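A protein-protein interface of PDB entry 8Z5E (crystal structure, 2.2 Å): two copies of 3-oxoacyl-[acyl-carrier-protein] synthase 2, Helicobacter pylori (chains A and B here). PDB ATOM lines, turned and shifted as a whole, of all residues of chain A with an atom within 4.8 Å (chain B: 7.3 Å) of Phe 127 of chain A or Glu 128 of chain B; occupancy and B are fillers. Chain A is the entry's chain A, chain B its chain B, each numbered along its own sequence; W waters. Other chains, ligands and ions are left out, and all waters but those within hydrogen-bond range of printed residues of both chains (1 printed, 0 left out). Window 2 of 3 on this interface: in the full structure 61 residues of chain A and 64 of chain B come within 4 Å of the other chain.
OG of Ser 123 of chain A touches CA of Glu 120 of chain B (3.5 Å).
N of Ser 123 of chain A touches CG2 of Val 202 of chain B (3.7 Å).
CD1 of Ile 124 of chain A touches CB of Phe 127 of chain B (3.6 Å).
Pro 201 of chain B touches Cys 126 of chain A.
Phe 127 of chain A touches Ile 124 of chain B (CB to CD1, 3.6 Å).
Phe 127 of chain A touches Glu 128 of chain B.
Phe 127 of chain B touches Glu 128 of chain A.
The backbone NH (N) of Val 202 of chain B lies within hydrogen-bond range of the side-chain carboxylate (OE2) of Glu 120 of chain B, 2.7 Å away.
Of chain B, only Ile 124 and Glu 128 come within 4 Å of Phe 127 of chain A.
Of chain A, only Phe 127 comes within 4 Å of Glu 128 of chain B.
Of the printed residues of chain A, Glu 120 of chain B touches Ser 123 (3.5 Å).
Of the printed residues of chain A, Val 202 of chain B touches Ser 123.
Of the printed residues of chain B, Glu 128 of chain A touches Phe 127.
Printed residues of chain A within 4 Å of Pro 201 of chain B: Cys 126 (3.9 Å).
Phe 125 of chain B touches none of the printed residues of chain A.
Phe 125 of chain A touches none of the printed residues of chain B.
The nearest printed residue of chain A that does not touch Glu 128 of chain B is Glu 128 of chain A (5.7 Å).
Ile 124 of chain A touches Phe 127 of chain B, and with the chains exchanged Phe 127 of chain A touches Ile 124 of chain B.
Phe 127 of chain A touches Glu 128 of chain B, and with the chains exchanged Glu 128 of chain A touches Phe 127 of chain B.
Positions printed for both chains: 123, 124, 125, 126, 127, 128, 129 and 130.
Water W1 lies within hydrogen-bond range of the side-chain carboxylate (OE2) of Glu 120 of chain B and the backbone carbonyl oxygen (O) of Ser 123 of chain A.
Of the 13 printed residues of chain B, 6 touch a printed residue of chain A.
Hydrophobic or aromatic side chains of chain B within 4 Å of the printed part of chain A: Ile 124, Phe 127, Pro 201 and Val 202.
Among the printed residues, 7 pairs touch across the chains.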
ATOM      1  N   SER A 123     -31.685 -20.877 -20.700  1.00  0.00           N
ATOM      2  CA  SER A 123     -31.736 -19.446 -21.095  1.00  0.00           C
ATOM      3  C   SER A 123     -30.306 -18.927 -21.269  1.00  0.00           C
ATOM      4  O   SER A 123     -30.037 -18.269 -22.290  1.00  0.00           O
ATOM      5  CB  SER A 123     -32.505 -18.629 -20.086  1.00  0.00           C
ATOM      6  OG  SER A 123     -33.848 -19.070 -19.991  1.00  0.00           O
ATOM      7  N   ILE A 124     -29.423 -19.245 -20.319  1.00  0.00           N
ATOM      8  CA  ILE A 124     -28.007 -18.772 -20.377  1.00  0.00           C
ATOM      9  C   ILE A 124     -27.299 -19.436 -21.565  1.00  0.00           C
ATOM     10  O   ILE A 124     -26.563 -18.730 -22.277  1.00  0.00           O
ATOM     11  CB  ILE A 124     -27.290 -19.044 -19.038  1.00  0.00           C
ATOM     12  CG1 ILE A 124     -28.031 -18.394 -17.867  1.00  0.00           C
ATOM     13  CG2 ILE A 124     -25.837 -18.605 -19.101  1.00  0.00           C
ATOM     14  CD1 ILE A 124     -27.461 -18.733 -16.510  1.00  0.00           C
ATOM     15  N   PHE A 125     -27.531 -20.733 -21.776  1.00  0.00           N
ATOM     16  CA  PHE A 125     -26.911 -21.453 -22.917  1.00  0.00           C
ATOM     17  C   PHE A 125     -27.265 -20.744 -24.228  1.00  0.00           C
ATOM     18  O   PHE A 125     -26.348 -20.444 -25.013  1.00  0.00           O
ATOM     19  CB  PHE A 125     -27.412 -22.896 -22.982  1.00  0.00           C
ATOM     20  CG  PHE A 125     -27.044 -23.776 -21.816  1.00  0.00           C
ATOM     21  CD1 PHE A 125     -26.179 -23.331 -20.829  1.00  0.00           C
ATOM     22  CD2 PHE A 125     -27.583 -25.046 -21.696  1.00  0.00           C
ATOM     23  CE1 PHE A 125     -25.853 -24.145 -19.757  1.00  0.00           C
ATOM     24  CE2 PHE A 125     -27.256 -25.859 -20.622  1.00  0.00           C
ATOM     25  CZ  PHE A 125     -26.391 -25.406 -19.655  1.00  0.00           C
ATOM     26  N   CYS A 126     -28.556 -20.482 -24.451  1.00  0.00           N
ATOM     27  CA  CYS A 126     -29.004 -19.852 -25.721  1.00  0.00           C
ATOM     28  C   CYS A 126     -28.394 -18.453 -25.839  1.00  0.00           C
ATOM     29  O   CYS A 126     -27.977 -18.083 -26.950  1.00  0.00           O
ATOM     30  CB  CYS A 126     -30.526 -19.767 -25.765  1.00  0.00           C
ATOM     31  SG  CYS A 126     -31.188 -19.264 -27.373  1.00  0.00           S
ATOM     32  N   PHE A 127     -28.338 -17.715 -24.731  1.00  0.00           N
ATOM     33  CA  PHE A 127     -27.820 -16.323 -24.754  1.00  0.00           C
ATOM     34  C   PHE A 127     -26.321 -16.310 -25.074  1.00  0.00           C
ATOM     35  O   PHE A 127     -25.890 -15.412 -25.815  1.00  0.00           O
ATOM     36  CB  PHE A 127     -28.092 -15.648 -23.409  1.00  0.00           C
ATOM     37  CG  PHE A 127     -27.557 -14.246 -23.273  1.00  0.00           C
ATOM     38  CD1 PHE A 127     -28.023 -13.225 -24.085  1.00  0.00           C
ATOM     39  CD2 PHE A 127     -26.585 -13.945 -22.333  1.00  0.00           C
ATOM     40  CE1 PHE A 127     -27.531 -11.935 -23.956  1.00  0.00           C
ATOM     41  CE2 PHE A 127     -26.094 -12.656 -22.206  1.00  0.00           C
ATOM     42  CZ  PHE A 127     -26.568 -11.654 -23.018  1.00  0.00           C
ATOM     43  N   GLU A 128     -25.557 -17.268 -24.541  1.00  0.00           N
ATOM     44  CA  GLU A 128     -24.077 -17.242 -24.715  1.00  0.00           C
ATOM     45  C   GLU A 128     -23.632 -17.986 -25.980  1.00  0.00           C
ATOM     46  O   GLU A 128     -22.687 -17.502 -26.627  1.00  0.00           O
ATOM     47  CB  GLU A 128     -23.387 -17.858 -23.496  1.00  0.00           C
ATOM     48  CG  GLU A 128     -23.089 -16.861 -22.392  1.00  0.00           C
ATOM     49  CD  GLU A 128     -22.022 -17.327 -21.416  1.00  0.00           C
ATOM     50  OE1 GLU A 128     -22.223 -18.378 -20.778  1.00  0.00           O
ATOM     51  OE2 GLU A 128     -20.987 -16.639 -21.299  1.00  0.00           O
ATOM     52  N   LYS A 129     -24.265 -19.113 -26.316  1.00  0.00           N
ATOM     53  CA  LYS A 129     -23.766 -19.924 -27.462  1.00  0.00           C
ATOM     54  C   LYS A 129     -24.875 -20.228 -28.478  1.00  0.00           C
ATOM     55  O   LYS A 129     -24.651 -21.107 -29.329  1.00  0.00           O
ATOM     56  CB  LYS A 129     -23.118 -21.206 -26.932  1.00  0.00           C
ATOM     57  CG  LYS A 129     -21.677 -21.037 -26.469  1.00  0.00           C
ATOM     58  CD  LYS A 129     -21.362 -21.769 -25.185  1.00  0.00           C
ATOM     59  CE  LYS A 129     -19.921 -21.600 -24.757  1.00  0.00           C
ATOM     60  NZ  LYS A 129     -18.983 -22.153 -25.763  1.00  0.00           N
ATOM     61  N   GLY A 130     -26.015 -19.539 -28.403  1.00  0.00           N
ATOM     62  CA  GLY A 130     -27.067 -19.723 -29.422  1.00  0.00           C
ATOM     63  C   GLY A 130     -28.039 -20.844 -29.102  1.00  0.00           C
ATOM     64  O   GLY A 130     -27.820 -21.559 -28.107  1.00  0.00           O
ATOM     65  N   GLU B 120     -36.375 -15.901 -18.611  1.00  0.00           N
ATOM     66  CA  GLU B 120     -35.174 -15.888 -19.432  1.00  0.00           C
ATOM     67  C   GLU B 120     -34.376 -14.610 -19.204  1.00  0.00           C
ATOM     68  O   GLU B 120     -33.158 -14.656 -18.987  1.00  0.00           O
ATOM     69  CB  GLU B 120     -35.580 -16.054 -20.904  1.00  0.00           C
ATOM     70  CG  GLU B 120     -34.497 -15.772 -21.944  1.00  0.00           C
ATOM     71  CD  GLU B 120     -35.037 -15.912 -23.368  1.00  0.00           C
ATOM     72  OE1 GLU B 120     -36.018 -15.212 -23.709  1.00  0.00           O
ATOM     73  OE2 GLU B 120     -34.483 -16.722 -24.146  1.00  0.00           O
ATOM     74  N   ASN B 122     -34.476 -12.383 -16.620  1.00  0.00           N
ATOM     75  CA  ASN B 122     -33.918 -12.217 -15.283  1.00  0.00           C
ATOM     76  C   ASN B 122     -32.870 -13.279 -14.991  1.00  0.00           C
ATOM     77  O   ASN B 122     -31.922 -13.013 -14.242  1.00  0.00           O
ATOM     78  CB  ASN B 122     -35.021 -12.239 -14.226  1.00  0.00           C
ATOM     79  CG  ASN B 122     -35.781 -10.923 -14.144  1.00  0.00           C
ATOM     80  OD1 ASN B 122     -35.395 -10.003 -13.422  1.00  0.00           O
ATOM     81  ND2 ASN B 122     -36.869 -10.836 -14.877  1.00  0.00           N
ATOM     82  N   SER B 123     -33.008 -14.470 -15.589  1.00  0.00           N
ATOM     83  CA  SER B 123     -31.956 -15.478 -15.477  1.00  0.00           C
ATOM     84  C   SER B 123     -30.634 -14.948 -16.017  1.00  0.00           C
ATOM     85  O   SER B 123     -29.566 -15.185 -15.432  1.00  0.00           O
ATOM     86  CB  SER B 123     -32.372 -16.746 -16.215  1.00  0.00           C
ATOM     87  OG  SER B 123     -33.471 -17.356 -15.542  1.00  0.00           O
ATOM     88  N   ILE B 124     -30.696 -14.216 -17.130  1.00  0.00           N
ATOM     89  CA  ILE B 124     -29.505 -13.662 -17.754  1.00  0.00           C
ATOM     90  C   ILE B 124     -28.981 -12.482 -16.949  1.00  0.00           C
ATOM     91  O   ILE B 124     -27.773 -12.369 -16.725  1.00  0.00           O
ATOM     92  CB  ILE B 124     -29.820 -13.284 -19.214  1.00  0.00           C
ATOM     93  CG1 ILE B 124     -29.897 -14.557 -20.067  1.00  0.00           C
ATOM     94  CG2 ILE B 124     -28.803 -12.312 -19.773  1.00  0.00           C
ATOM     95  CD1 ILE B 124     -30.761 -14.419 -21.283  1.00  0.00           C
ATOM     96  N   PHE B 125     -29.875 -11.592 -16.497  1.00  0.00           N
ATOM     97  CA  PHE B 125     -29.481 -10.542 -15.553  1.00  0.00           C
ATOM     98  C   PHE B 125     -28.702 -11.117 -14.372  1.00  0.00           C
ATOM     99  O   PHE B 125     -27.660 -10.580 -13.971  1.00  0.00           O
ATOM    100  CB  PHE B 125     -30.700  -9.801 -15.006  1.00  0.00           C
ATOM    101  CG  PHE B 125     -31.483  -9.039 -16.027  1.00  0.00           C
ATOM    102  CD1 PHE B 125     -30.959  -8.758 -17.280  1.00  0.00           C
ATOM    103  CD2 PHE B 125     -32.773  -8.597 -15.720  1.00  0.00           C
ATOM    104  CE1 PHE B 125     -31.705  -8.056 -18.213  1.00  0.00           C
ATOM    105  CE2 PHE B 125     -33.525  -7.894 -16.648  1.00  0.00           C
ATOM    106  CZ  PHE B 125     -32.989  -7.622 -17.893  1.00  0.00           C
ATOM    107  N   CYS B 126     -29.222 -12.189 -13.773  1.00  0.00           N
ATOM    108  CA  CYS B 126     -28.596 -12.735 -12.575  1.00  0.00           C
ATOM    109  C   CYS B 126     -27.242 -13.346 -12.888  1.00  0.00           C
ATOM    110  O   CYS B 126     -26.318 -13.249 -12.076  1.00  0.00           O
ATOM    111  CB  CYS B 126     -29.503 -13.787 -11.933  1.00  0.00           C
ATOM    112  SG  CYS B 126     -29.019 -14.208 -10.231  1.00  0.00           S
ATOM    113  N   PHE B 127     -27.108 -13.964 -14.062  1.00  0.00           N
ATOM    114  CA  PHE B 127     -25.859 -14.585 -14.461  1.00  0.00           C
ATOM    115  C   PHE B 127     -24.790 -13.560 -14.839  1.00  0.00           C
ATOM    116  O   PHE B 127     -23.598 -13.807 -14.619  1.00  0.00           O
ATOM    117  CB  PHE B 127     -26.132 -15.548 -15.614  1.00  0.00           C
ATOM    118  CG  PHE B 127     -24.899 -16.063 -16.290  1.00  0.00           C
ATOM    119  CD1 PHE B 127     -24.174 -17.106 -15.742  1.00  0.00           C
ATOM    120  CD2 PHE B 127     -24.484 -15.523 -17.504  1.00  0.00           C
ATOM    121  CE1 PHE B 127     -23.040 -17.585 -16.382  1.00  0.00           C
ATOM    122  CE2 PHE B 127     -23.359 -16.002 -18.143  1.00  0.00           C
ATOM    123  CZ  PHE B 127     -22.637 -17.031 -17.575  1.00  0.00           C
ATOM    124  N   GLU B 128     -25.180 -12.412 -15.391  1.00  0.00           N
ATOM    125  CA  GLU B 128     -24.205 -11.428 -15.843  1.00  0.00           C
ATOM    126  C   GLU B 128     -23.839 -10.412 -14.766  1.00  0.00           C
ATOM    127  O   GLU B 128     -22.674 -10.011 -14.678  1.00  0.00           O
ATOM    128  CB  GLU B 128     -24.736 -10.701 -17.082  1.00  0.00           C
ATOM    129  CG  GLU B 128     -24.896 -11.615 -18.285  1.00  0.00           C
ATOM    130  CD  GLU B 128     -24.256 -11.039 -19.534  1.00  0.00           C
ATOM    131  OE1 GLU B 128     -24.760 -10.010 -20.040  1.00  0.00           O
ATOM    132  OE2 GLU B 128     -23.249 -11.613 -20.012  1.00  0.00           O
ATOM    133  N   LYS B 129     -24.800  -9.985 -13.942  1.00  0.00           N
ATOM    134  CA  LYS B 129     -24.596  -8.879 -13.014  1.00  0.00           C
ATOM    135  C   LYS B 129     -24.881  -9.246 -11.560  1.00  0.00           C
ATOM    136  O   LYS B 129     -24.833  -8.362 -10.693  1.00  0.00           O
ATOM    137  CB  LYS B 129     -25.465  -7.684 -13.427  1.00  0.00           C
ATOM    138  CG  LYS B 129     -25.009  -7.001 -14.720  1.00  0.00           C
ATOM    139  CD  LYS B 129     -26.156  -6.859 -15.722  1.00  0.00           C
ATOM    140  CE  LYS B 129     -27.107  -5.741 -15.319  1.00  0.00           C
ATOM    141  NZ  LYS B 129     -28.320  -5.605 -16.190  1.00  0.00           N
ATOM    142  N   GLY B 130     -25.177 -10.513 -11.264  1.00  0.00           N
ATOM    143  CA  GLY B 130     -25.499 -10.937  -9.917  1.00  0.00           C
ATOM    144  C   GLY B 130     -26.964 -10.759  -9.539  1.00  0.00           C
ATOM    145  O   GLY B 130     -27.739 -10.101 -10.238  1.00  0.00           O
ATOM    146  N   LYS B 133     -29.440  -7.539  -9.599  1.00  0.00           N
ATOM    147  CA  LYS B 133     -30.060  -7.056 -10.817  1.00  0.00           C
ATOM    148  C   LYS B 133     -31.328  -7.818 -11.185  1.00  0.00           C
ATOM    149  O   LYS B 133     -31.843  -7.638 -12.290  1.00  0.00           O
ATOM    150  CB  LYS B 133     -29.067  -7.107 -11.971  1.00  0.00           C
ATOM    151  CG  LYS B 133     -28.857  -5.731 -12.554  1.00  0.00           C
ATOM    152  CD  LYS B 133     -28.396  -4.720 -11.500  1.00  0.00           C
ATOM    153  CE  LYS B 133     -26.908  -4.864 -11.216  1.00  0.00           C
ATOM    154  NZ  LYS B 133     -26.408  -3.757 -10.360  1.00  0.00           N
ATOM    155  N   PRO B 201     -36.201 -16.283 -27.416  1.00  0.00           N
ATOM    156  CA  PRO B 201     -35.112 -17.183 -27.839  1.00  0.00           C
ATOM    157  C   PRO B 201     -35.170 -18.559 -27.192  1.00  0.00           C
ATOM    158  O   PRO B 201     -35.170 -19.572 -27.907  1.00  0.00           O
ATOM    159  CB  PRO B 201     -33.845 -16.401 -27.454  1.00  0.00           C
ATOM    160  CG  PRO B 201     -34.257 -14.979 -27.486  1.00  0.00           C
ATOM    161  CD  PRO B 201     -35.689 -14.960 -27.009  1.00  0.00           C
ATOM    162  N   VAL B 202     -35.238 -18.644 -25.862  1.00  0.00           N
ATOM    163  CA  VAL B 202     -35.250 -19.975 -25.271  1.00  0.00           C
ATOM    164  C   VAL B 202     -36.560 -20.702 -25.573  1.00  0.00           C
ATOM    165  O   VAL B 202     -36.597 -21.937 -25.544  1.00  0.00           O
ATOM    166  CB  VAL B 202     -34.976 -19.918 -23.755  1.00  0.00           C
ATOM    167  CG1 VAL B 202     -36.278 -19.691 -22.961  1.00  0.00           C
ATOM    168  CG2 VAL B 202     -34.268 -21.207 -23.303  1.00  0.00           C
HETATM  169  O   HOH W   1     -31.869 -16.934 -23.947  1.00  0.00           O
